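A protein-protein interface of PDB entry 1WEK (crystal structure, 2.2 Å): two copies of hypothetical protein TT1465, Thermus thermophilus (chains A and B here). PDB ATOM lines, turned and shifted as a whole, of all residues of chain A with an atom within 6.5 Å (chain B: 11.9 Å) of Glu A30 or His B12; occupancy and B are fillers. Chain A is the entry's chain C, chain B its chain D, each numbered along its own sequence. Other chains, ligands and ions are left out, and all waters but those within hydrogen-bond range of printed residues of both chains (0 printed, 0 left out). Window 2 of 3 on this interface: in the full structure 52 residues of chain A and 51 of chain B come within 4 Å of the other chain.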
ATOM      1  N   PHE A  25     -34.887  10.413  22.267  1.00  0.00           N
ATOM      2  CA  PHE A  25     -33.752  11.293  22.559  1.00  0.00           C
ATOM      3  C   PHE A  25     -33.256  11.962  21.274  1.00  0.00           C
ATOM      4  O   PHE A  25     -33.062  13.182  21.214  1.00  0.00           O
ATOM      5  CB  PHE A  25     -32.601  10.507  23.185  1.00  0.00           C
ATOM      6  CG  PHE A  25     -32.811  10.165  24.638  1.00  0.00           C
ATOM      7  CD1 PHE A  25     -32.914   8.840  25.046  1.00  0.00           C
ATOM      8  CD2 PHE A  25     -32.836  11.165  25.604  1.00  0.00           C
ATOM      9  CE1 PHE A  25     -33.029   8.511  26.389  1.00  0.00           C
ATOM     10  CE2 PHE A  25     -32.951  10.849  26.960  1.00  0.00           C
ATOM     11  CZ  PHE A  25     -33.046   9.517  27.351  1.00  0.00           C
ATOM     12  N   VAL A  26     -33.061  11.151  20.244  1.00  0.00           N
ATOM     13  CA  VAL A  26     -32.592  11.661  18.976  1.00  0.00           C
ATOM     14  C   VAL A  26     -33.432  12.833  18.500  1.00  0.00           C
ATOM     15  O   VAL A  26     -32.906  13.906  18.217  1.00  0.00           O
ATOM     16  CB  VAL A  26     -32.612  10.564  17.915  1.00  0.00           C
ATOM     17  CG1 VAL A  26     -32.431  11.168  16.541  1.00  0.00           C
ATOM     18  CG2 VAL A  26     -31.511   9.559  18.215  1.00  0.00           C
ATOM     19  N   GLU A  27     -34.739  12.614  18.418  1.00  0.00           N
ATOM     20  CA  GLU A  27     -35.656  13.640  17.968  1.00  0.00           C
ATOM     21  C   GLU A  27     -35.603  14.823  18.919  1.00  0.00           C
ATOM     22  O   GLU A  27     -35.550  15.975  18.480  1.00  0.00           O
ATOM     23  CB  GLU A  27     -37.067  13.051  17.869  1.00  0.00           C
ATOM     24  CG  GLU A  27     -37.219  12.105  16.673  1.00  0.00           C
ATOM     25  CD  GLU A  27     -38.350  11.095  16.831  1.00  0.00           C
ATOM     26  OE1 GLU A  27     -39.486  11.512  17.154  1.00  0.00           O
ATOM     27  OE2 GLU A  27     -38.107   9.880  16.623  1.00  0.00           O
ATOM     28  N   GLY A  28     -35.591  14.528  20.219  1.00  0.00           N
ATOM     29  CA  GLY A  28     -35.522  15.569  21.225  1.00  0.00           C
ATOM     30  C   GLY A  28     -34.275  16.425  21.061  1.00  0.00           C
ATOM     31  O   GLY A  28     -34.355  17.658  21.047  1.00  0.00           O
ATOM     32  N   PHE A  29     -33.111  15.788  20.938  1.00  0.00           N
ATOM     33  CA  PHE A  29     -31.872  16.541  20.770  1.00  0.00           C
ATOM     34  C   PHE A  29     -31.924  17.379  19.491  1.00  0.00           C
ATOM     35  O   PHE A  29     -31.458  18.521  19.464  1.00  0.00           O
ATOM     36  CB  PHE A  29     -30.660  15.599  20.737  1.00  0.00           C
ATOM     37  CG  PHE A  29     -30.444  14.838  22.020  1.00  0.00           C
ATOM     38  CD1 PHE A  29     -30.688  15.439  23.256  1.00  0.00           C
ATOM     39  CD2 PHE A  29     -29.941  13.544  21.997  1.00  0.00           C
ATOM     40  CE1 PHE A  29     -30.428  14.764  24.456  1.00  0.00           C
ATOM     41  CE2 PHE A  29     -29.680  12.862  23.192  1.00  0.00           C
ATOM     42  CZ  PHE A  29     -29.923  13.474  24.423  1.00  0.00           C
ATOM     43  N   GLU A  30     -32.509  16.824  18.435  1.00  0.00           N
ATOM     44  CA  GLU A  30     -32.611  17.558  17.174  1.00  0.00           C
ATOM     45  C   GLU A  30     -33.497  18.788  17.303  1.00  0.00           C
ATOM     46  O   GLU A  30     -33.096  19.890  16.959  1.00  0.00           O
ATOM     47  CB  GLU A  30     -33.194  16.685  16.063  1.00  0.00           C
ATOM     48  CG  GLU A  30     -32.433  15.428  15.774  1.00  0.00           C
ATOM     49  CD  GLU A  30     -32.985  14.709  14.565  1.00  0.00           C
ATOM     50  OE1 GLU A  30     -34.222  14.644  14.420  1.00  0.00           O
ATOM     51  OE2 GLU A  30     -32.185  14.199  13.759  1.00  0.00           O
ATOM     52  N   THR A  31     -34.714  18.587  17.791  1.00  0.00           N
ATOM     53  CA  THR A  31     -35.640  19.687  17.925  1.00  0.00           C
ATOM     54  C   THR A  31     -35.063  20.849  18.721  1.00  0.00           C
ATOM     55  O   THR A  31     -35.052  21.985  18.243  1.00  0.00           O
ATOM     56  CB  THR A  31     -36.954  19.227  18.589  1.00  0.00           C
ATOM     57  OG1 THR A  31     -37.601  18.262  17.749  1.00  0.00           O
ATOM     58  CG2 THR A  31     -37.888  20.399  18.795  1.00  0.00           C
ATOM     59  N   LEU A  32     -34.567  20.560  19.920  1.00  0.00           N
ATOM     60  CA  LEU A  32     -34.030  21.592  20.801  1.00  0.00           C
ATOM     61  C   LEU A  32     -32.718  22.243  20.380  1.00  0.00           C
ATOM     62  O   LEU A  32     -32.569  23.465  20.470  1.00  0.00           O
ATOM     63  CB  LEU A  32     -33.889  21.024  22.216  1.00  0.00           C
ATOM     64  CG  LEU A  32     -35.019  21.308  23.218  1.00  0.00           C
ATOM     65  CD1 LEU A  32     -36.356  21.215  22.548  1.00  0.00           C
ATOM     66  CD2 LEU A  32     -34.925  20.340  24.385  1.00  0.00           C
ATOM     67  N   SER A  33     -31.767  21.438  19.914  1.00  0.00           N
ATOM     68  CA  SER A  33     -30.461  21.961  19.511  1.00  0.00           C
ATOM     69  C   SER A  33     -30.510  22.901  18.306  1.00  0.00           C
ATOM     70  O   SER A  33     -29.639  23.760  18.152  1.00  0.00           O
ATOM     71  CB  SER A  33     -29.500  20.806  19.203  1.00  0.00           C
ATOM     72  OG  SER A  33     -29.975  20.024  18.120  1.00  0.00           O
ATOM     73  N   GLU A  34     -31.512  22.765  17.442  1.00  0.00           N
ATOM     74  CA  GLU A  34     -31.518  23.651  16.296  1.00  0.00           C
ATOM     75  C   GLU A  34     -32.067  25.039  16.631  1.00  0.00           C
ATOM     76  O   GLU A  34     -31.909  25.980  15.840  1.00  0.00           O
ATOM     77  CB  GLU A  34     -32.256  23.017  15.112  1.00  0.00           C
ATOM     78  CG  GLU A  34     -33.762  23.050  15.179  1.00  0.00           C
ATOM     79  CD  GLU A  34     -34.380  22.490  13.903  1.00  0.00           C
ATOM     80  OE1 GLU A  34     -34.276  21.256  13.687  1.00  0.00           O
ATOM     81  OE2 GLU A  34     -34.950  23.285  13.109  1.00  0.00           O
ATOM     82  N   LEU A  35     -32.692  25.173  17.805  1.00  0.00           N
ATOM     83  CA  LEU A  35     -33.207  26.476  18.235  1.00  0.00           C
ATOM     84  C   LEU A  35     -32.006  27.373  18.532  1.00  0.00           C
ATOM     85  O   LEU A  35     -30.998  26.916  19.059  1.00  0.00           O
ATOM     86  CB  LEU A  35     -34.050  26.346  19.496  1.00  0.00           C
ATOM     87  CG  LEU A  35     -35.383  25.607  19.370  1.00  0.00           C
ATOM     88  CD1 LEU A  35     -36.065  25.553  20.750  1.00  0.00           C
ATOM     89  CD2 LEU A  35     -36.264  26.326  18.350  1.00  0.00           C
ATOM     90  N   TYR A 131     -29.857  21.738  27.270  1.00  0.00           N
ATOM     91  CA  TYR A 131     -29.613  23.027  26.627  1.00  0.00           C
ATOM     92  C   TYR A 131     -29.988  24.200  27.533  1.00  0.00           C
ATOM     93  O   TYR A 131     -30.069  25.344  27.081  1.00  0.00           O
ATOM     94  CB  TYR A 131     -30.400  23.115  25.311  1.00  0.00           C
ATOM     95  CG  TYR A 131     -30.198  21.908  24.427  1.00  0.00           C
ATOM     96  CD1 TYR A 131     -31.190  20.945  24.295  1.00  0.00           C
ATOM     97  CD2 TYR A 131     -28.982  21.702  23.758  1.00  0.00           C
ATOM     98  CE1 TYR A 131     -30.988  19.801  23.518  1.00  0.00           C
ATOM     99  CE2 TYR A 131     -28.768  20.558  22.987  1.00  0.00           C
ATOM    100  CZ  TYR A 131     -29.775  19.615  22.873  1.00  0.00           C
ATOM    101  OH  TYR A 131     -29.561  18.473  22.136  1.00  0.00           O
ATOM    102  N   LEU B   6     -21.246  14.518  31.609  1.00  0.00           N
ATOM    103  CA  LEU B   6     -21.943  13.394  31.001  1.00  0.00           C
ATOM    104  C   LEU B   6     -23.051  13.824  30.042  1.00  0.00           C
ATOM    105  O   LEU B   6     -23.004  13.523  28.850  1.00  0.00           O
ATOM    106  CB  LEU B   6     -22.553  12.517  32.089  1.00  0.00           C
ATOM    107  CG  LEU B   6     -22.665  10.999  31.865  1.00  0.00           C
ATOM    108  CD1 LEU B   6     -23.859  10.479  32.665  1.00  0.00           C
ATOM    109  CD2 LEU B   6     -22.841  10.653  30.401  1.00  0.00           C
ATOM    110  N   ILE B   7     -24.042  14.533  30.583  1.00  0.00           N
ATOM    111  CA  ILE B   7     -25.190  14.980  29.815  1.00  0.00           C
ATOM    112  C   ILE B   7     -24.867  15.806  28.586  1.00  0.00           C
ATOM    113  O   ILE B   7     -25.519  15.658  27.562  1.00  0.00           O
ATOM    114  CB  ILE B   7     -26.173  15.766  30.705  1.00  0.00           C
ATOM    115  CG1 ILE B   7     -26.633  14.877  31.860  1.00  0.00           C
ATOM    116  CG2 ILE B   7     -27.369  16.234  29.882  1.00  0.00           C
ATOM    117  CD1 ILE B   7     -27.191  13.545  31.417  1.00  0.00           C
ATOM    118  N   ASP B   8     -23.864  16.668  28.673  1.00  0.00           N
ATOM    119  CA  ASP B   8     -23.506  17.491  27.526  1.00  0.00           C
ATOM    120  C   ASP B   8     -22.800  16.703  26.429  1.00  0.00           C
ATOM    121  O   ASP B   8     -22.576  17.215  25.326  1.00  0.00           O
ATOM    122  CB  ASP B   8     -22.648  18.672  27.976  1.00  0.00           C
ATOM    123  CG  ASP B   8     -23.342  19.521  29.036  1.00  0.00           C
ATOM    124  OD1 ASP B   8     -23.273  19.170  30.231  1.00  0.00           O
ATOM    125  OD2 ASP B   8     -23.978  20.526  28.672  1.00  0.00           O
ATOM    126  N   GLN B   9     -22.453  15.452  26.711  1.00  0.00           N
ATOM    127  CA  GLN B   9     -21.789  14.648  25.685  1.00  0.00           C
ATOM    128  C   GLN B   9     -22.800  13.923  24.798  1.00  0.00           C
ATOM    129  O   GLN B   9     -22.433  13.291  23.819  1.00  0.00           O
ATOM    130  CB  GLN B   9     -20.805  13.656  26.315  1.00  0.00           C
ATOM    131  CG  GLN B   9     -19.625  14.361  26.973  1.00  0.00           C
ATOM    132  CD  GLN B   9     -18.454  13.445  27.261  1.00  0.00           C
ATOM    133  OE1 GLN B   9     -17.503  13.840  27.935  1.00  0.00           O
ATOM    134  NE2 GLN B   9     -18.509  12.220  26.746  1.00  0.00           N
ATOM    135  N   LEU B  10     -24.079  14.028  25.141  1.00  0.00           N
ATOM    136  CA  LEU B  10     -25.120  13.402  24.337  1.00  0.00           C
ATOM    137  C   LEU B  10     -25.441  14.295  23.140  1.00  0.00           C
ATOM    138  O   LEU B  10     -25.613  15.518  23.279  1.00  0.00           O
ATOM    139  CB  LEU B  10     -26.379  13.185  25.174  1.00  0.00           C
ATOM    140  CG  LEU B  10     -26.196  12.234  26.347  1.00  0.00           C
ATOM    141  CD1 LEU B  10     -27.395  12.310  27.281  1.00  0.00           C
ATOM    142  CD2 LEU B  10     -25.984  10.827  25.805  1.00  0.00           C
ATOM    143  N   HIS B  11     -25.506  13.671  21.970  1.00  0.00           N
ATOM    144  CA  HIS B  11     -25.813  14.341  20.700  1.00  0.00           C
ATOM    145  C   HIS B  11     -26.601  13.313  19.883  1.00  0.00           C
ATOM    146  O   HIS B  11     -26.373  12.105  20.017  1.00  0.00           O
ATOM    147  CB  HIS B  11     -24.515  14.715  19.975  1.00  0.00           C
ATOM    148  CG  HIS B  11     -23.641  15.655  20.748  1.00  0.00           C
ATOM    149  ND1 HIS B  11     -23.683  17.022  20.576  1.00  0.00           N
ATOM    150  CD2 HIS B  11     -22.742  15.430  21.734  1.00  0.00           C
ATOM    151  CE1 HIS B  11     -22.849  17.598  21.422  1.00  0.00           C
ATOM    152  NE2 HIS B  11     -22.265  16.655  22.137  1.00  0.00           N
ATOM    153  N   HIS B  12     -27.509  13.771  19.027  1.00  0.00           N
ATOM    154  CA  HIS B  12     -28.315  12.830  18.259  1.00  0.00           C
ATOM    155  C   HIS B  12     -27.515  12.046  17.239  1.00  0.00           C
ATOM    156  O   HIS B  12     -27.964  11.000  16.768  1.00  0.00           O
ATOM    157  CB  HIS B  12     -29.491  13.548  17.584  1.00  0.00           C
ATOM    158  CG  HIS B  12     -29.088  14.482  16.488  1.00  0.00           C
ATOM    159  ND1 HIS B  12     -29.139  14.132  15.157  1.00  0.00           N
ATOM    160  CD2 HIS B  12     -28.638  15.758  16.524  1.00  0.00           C
ATOM    161  CE1 HIS B  12     -28.741  15.154  14.420  1.00  0.00           C
ATOM    162  NE2 HIS B  12     -28.431  16.152  15.227  1.00  0.00           N
ATOM    163  N   GLU B  13     -26.320  12.535  16.917  1.00  0.00           N
ATOM    164  CA  GLU B  13     -25.467  11.859  15.947  1.00  0.00           C
ATOM    165  C   GLU B  13     -24.410  10.951  16.590  1.00  0.00           C
ATOM    166  O   GLU B  13     -23.797  10.145  15.897  1.00  0.00           O
ATOM    167  CB  GLU B  13     -24.793  12.887  15.028  1.00  0.00           C
ATOM    168  CG  GLU B  13     -25.778  13.654  14.146  1.00  0.00           C
ATOM    169  CD  GLU B  13     -25.156  14.859  13.447  1.00  0.00           C
ATOM    170  OE1 GLU B  13     -24.570  15.725  14.143  1.00  0.00           O
ATOM    171  OE2 GLU B  13     -25.265  14.946  12.201  1.00  0.00           O
ATOM    172  N   ASP B  14     -24.197  11.076  17.902  1.00  0.00           N
ATOM    173  CA  ASP B  14     -23.213  10.236  18.596  1.00  0.00           C
ATOM    174  C   ASP B  14     -23.851   8.921  19.058  1.00  0.00           C
ATOM    175  O   ASP B  14     -24.082   8.701  20.248  1.00  0.00           O
ATOM    176  CB  ASP B  14     -22.623  10.982  19.798  1.00  0.00           C
ATOM    177  CG  ASP B  14     -21.776  12.186  19.384  1.00  0.00           C
ATOM    178  OD1 ASP B  14     -21.444  12.300  18.180  1.00  0.00           O
ATOM    179  OD2 ASP B  14     -21.433  13.010  20.265  1.00  0.00           O
ATOM    180  N   SER B  15     -24.132   8.053  18.095  1.00  0.00           N
ATOM    181  CA  SER B  15     -24.770   6.768  18.336  1.00  0.00           C
ATOM    182  C   SER B  15     -24.295   5.918  19.516  1.00  0.00           C
ATOM    183  O   SER B  15     -25.122   5.331  20.214  1.00  0.00           O
ATOM    184  CB  SER B  15     -24.692   5.921  17.068  1.00  0.00           C
ATOM    185  OG  SER B  15     -25.391   6.536  16.004  1.00  0.00           O
ATOM    186  N   TRP B  16     -22.982   5.852  19.746  1.00  0.00           N
ATOM    187  CA  TRP B  16     -22.442   5.011  20.811  1.00  0.00           C
ATOM    188  C   TRP B  16     -22.895   5.366  22.207  1.00  0.00           C
ATOM    189  O   TRP B  16     -23.204   4.475  23.000  1.00  0.00           O
ATOM    190  CB  TRP B  16     -20.904   4.963  20.750  1.00  0.00           C
ATOM    191  CG  TRP B  16     -20.200   6.274  20.967  1.00  0.00           C
ATOM    192  CD1 TRP B  16     -19.609   6.713  22.122  1.00  0.00           C
ATOM    193  CD2 TRP B  16     -19.948   7.282  19.981  1.00  0.00           C
ATOM    194  NE1 TRP B  16     -18.991   7.925  21.912  1.00  0.00           N
ATOM    195  CE2 TRP B  16     -19.185   8.298  20.606  1.00  0.00           C
ATOM    196  CE3 TRP B  16     -20.290   7.426  18.626  1.00  0.00           C
ATOM    197  CZ2 TRP B  16     -18.758   9.441  19.922  1.00  0.00           C
ATOM    198  CZ3 TRP B  16     -19.865   8.567  17.944  1.00  0.00           C
ATOM    199  CH2 TRP B  16     -19.107   9.559  18.596  1.00  0.00           C
ATOM    200  N   ARG B  17     -22.940   6.658  22.517  1.00  0.00           N
ATOM    201  CA  ARG B  17     -23.380   7.074  23.842  1.00  0.00           C
ATOM    202  C   ARG B  17     -24.851   6.716  24.061  1.00  0.00           C
ATOM    203  O   ARG B  17     -25.280   6.451  25.189  1.00  0.00           O
ATOM    204  CB  ARG B  17     -23.117   8.569  24.023  1.00  0.00           C
ATOM    205  CG  ARG B  17     -21.621   8.872  23.909  1.00  0.00           C
ATOM    206  CD  ARG B  17     -21.250  10.158  24.593  1.00  0.00           C
ATOM    207  NE  ARG B  17     -20.792  11.172  23.650  1.00  0.00           N
ATOM    208  CZ  ARG B  17     -19.520  11.408  23.337  1.00  0.00           C
ATOM    209  NH1 ARG B  17     -18.542  10.704  23.883  1.00  0.00           N
ATOM    210  NH2 ARG B  17     -19.233  12.378  22.485  1.00  0.00           N
ATOM    211  N   LEU B  18     -25.616   6.679  22.976  1.00  0.00           N
ATOM    212  CA  LEU B  18     -27.031   6.307  23.060  1.00  0.00           C
ATOM    213  C   LEU B  18     -27.116   4.780  23.220  1.00  0.00           C
ATOM    214  O   LEU B  18     -28.073   4.257  23.793  1.00  0.00           O
ATOM    215  CB  LEU B  18     -27.787   6.741  21.796  1.00  0.00           C
ATOM    216  CG  LEU B  18     -28.101   8.222  21.590  1.00  0.00           C
ATOM    217  CD1 LEU B  18     -28.682   8.418  20.199  1.00  0.00           C
ATOM    218  CD2 LEU B  18     -29.107   8.696  22.646  1.00  0.00           C
ATOM    219  N   PHE B  19     -26.114   4.061  22.715  1.00  0.00           N
ATOM    220  CA  PHE B  19     -26.126   2.607  22.861  1.00  0.00           C
ATOM    221  C   PHE B  19     -25.710   2.209  24.272  1.00  0.00           C
ATOM    222  O   PHE B  19     -26.072   1.134  24.743  1.00  0.00           O
ATOM    223  CB  PHE B  19     -25.230   1.950  21.819  1.00  0.00           C
ATOM    224  CG  PHE B  19     -25.955   1.576  20.545  1.00  0.00           C
ATOM    225  CD1 PHE B  19     -26.592   0.351  20.425  1.00  0.00           C
ATOM    226  CD2 PHE B  19     -25.999   2.448  19.469  1.00  0.00           C
ATOM    227  CE1 PHE B  19     -27.262   0.001  19.248  1.00  0.00           C
ATOM    228  CE2 PHE B  19     -26.664   2.110  18.291  1.00  0.00           C
ATOM    229  CZ  PHE B  19     -27.295   0.886  18.179  1.00  0.00           C
ATOM    230  N   ARG B  20     -24.960   3.080  24.948  1.00  0.00           N
ATOM    231  CA  ARG B  20     -24.547   2.821  26.333  1.00  0.00           C
ATOM    232  C   ARG B  20     -25.789   2.950  27.203  1.00  0.00           C
ATOM    233  O   ARG B  20     -25.925   2.278  28.226  1.00  0.00           O
ATOM    234  CB  ARG B  20     -23.500   3.840  26.809  1.00  0.00           C
ATOM    235  CG  ARG B  20     -23.261   3.821  28.332  1.00  0.00           C
ATOM    236  CD  ARG B  20     -22.579   2.525  28.768  1.00  0.00           C
ATOM    237  NE  ARG B  20     -22.472   2.393  30.224  1.00  0.00           N
ATOM    238  CZ  ARG B  20     -21.378   1.985  30.861  1.00  0.00           C
ATOM    239  NH1 ARG B  20     -20.278   1.674  30.182  1.00  0.00           N
ATOM    240  NH2 ARG B  20     -21.388   1.869  32.173  1.00  0.00           N
ATOM    241  N   ILE B  21     -26.680   3.854  26.807  1.00  0.00           N
ATOM    242  CA  ILE B  21     -27.927   4.033  27.531  1.00  0.00           C
ATOM    243  C   ILE B  21     -28.721   2.738  27.354  1.00  0.00           C
ATOM    244  O   ILE B  21     -29.318   2.240  28.297  1.00  0.00           O
ATOM    245  CB  ILE B  21     -28.731   5.232  26.977  1.00  0.00           C
ATOM    246  CG1 ILE B  21     -28.077   6.540  27.462  1.00  0.00           C
ATOM    247  CG2 ILE B  21     -30.201   5.116  27.400  1.00  0.00           C
ATOM    248  CD1 ILE B  21     -28.620   7.800  26.831  1.00  0.00           C
ATOM    249  N   TYR B 120     -25.900   6.663  33.685  1.00  0.00           N
ATOM    250  CA  TYR B 120     -27.043   7.540  33.555  1.00  0.00           C
ATOM    251  C   TYR B 120     -28.041   7.534  34.708  1.00  0.00           C
ATOM    252  O   TYR B 120     -28.705   6.537  34.991  1.00  0.00           O
ATOM    253  CB  TYR B 120     -27.734   7.261  32.208  1.00  0.00           C
ATOM    254  CG  TYR B 120     -26.835   7.613  31.035  1.00  0.00           C
ATOM    255  CD1 TYR B 120     -25.996   6.660  30.459  1.00  0.00           C
ATOM    256  CD2 TYR B 120     -26.767   8.931  30.551  1.00  0.00           C
ATOM    257  CE1 TYR B 120     -25.108   7.000  29.436  1.00  0.00           C
ATOM    258  CE2 TYR B 120     -25.885   9.285  29.542  1.00  0.00           C
ATOM    259  CZ  TYR B 120     -25.057   8.314  28.991  1.00  0.00           C
ATOM    260  OH  TYR B 120     -24.158   8.665  28.020  1.00  0.00           O
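Leu B18 touches Phe A25 (CD2 to CB, 3.97 Å).
His B12 touches Val A26.
Val A26 touches Leu B18 (CG2 to CD1, 3.6 Å).
CB of Leu B10 touches CZ of Phe A29 (3.6 Å).
C of His B11 touches CD2 of Phe A29, at 3.96 Å.
Phe A29 touches His B12.
Printed residues of chain B within 4 Å of Phe A25: Leu B18.
Val A26 touches just these residues of chain B: His B12 (3.5 Å) and Leu B18 (3.6 Å).
No residue of chain B comes within 4 Å of Glu A27.
Gly A28 touches none of the printed residues of chain B.
Of chain B, only Leu B10 (3.6 Å), His B11 (3.96 Å) and His B12 (3.8 Å) come within 4 Å of Phe A29.
Printed residues of chain B within 4 Å of Glu A30: His B12 (3.4 Å).
No residue of chain B comes within 4 Å of Thr A31.
No residue of chain B comes within 4 Å of Glu A34.
No residue of chain B comes within 4 Å of Leu A35.
Of the printed residues of chain A, His B11 touches Phe A29.
Trp B16 touches none of the printed residues of chain A.
Of the printed residues of chain A, Leu B18 touches Phe A25 (3.97 Å) and Val A26 (3.6 Å).
The nearest residue of chain B that does not touch Glu A30 is Glu B13 (6.4 Å).
The nearest printed residue of chain A that does not touch Leu B18 is Phe A29 (4.2 Å).
The backbone carbonyl oxygen (O) of Phe A29 is in hydrogen-bond range of the side-chain hydroxyl (OG) of Ser A33 (2.5 Å).
The backbone carbonyl oxygen (O) of Phe A29 lies within hydrogen-bond range of the side-chain hydroxyl (OH) of Tyr A131, at 3.3 Å.
O of Glu A30 lies within hydrogen-bond range of OG of Ser A33 (3.3 Å).
NE2 of His B11 sits at hydrogen-bond distance from O of Asp B8.
OE2 of Glu A30 is in hydrogen-bond range of ND1 of His B12, at 3.4 Å.
No position is printed for both chains.
Hydrophobic or aromatic side chains of chain B within 4 Å of the printed part of chain A: Leu B10, His B12 and Leu B18.
Hydrophobic or aromatic side chains of chain A within 4 Å of the printed part of chain B: Phe A25, Val A26 and Phe A29.
Along chain A the printed residues that touch a printed residue of chain B span positions 25 to 30.
Among the printed residues, no Asp or Glu carboxylate lies within 4 Å of a Lys or Arg side-chain nitrogen of the other chain.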
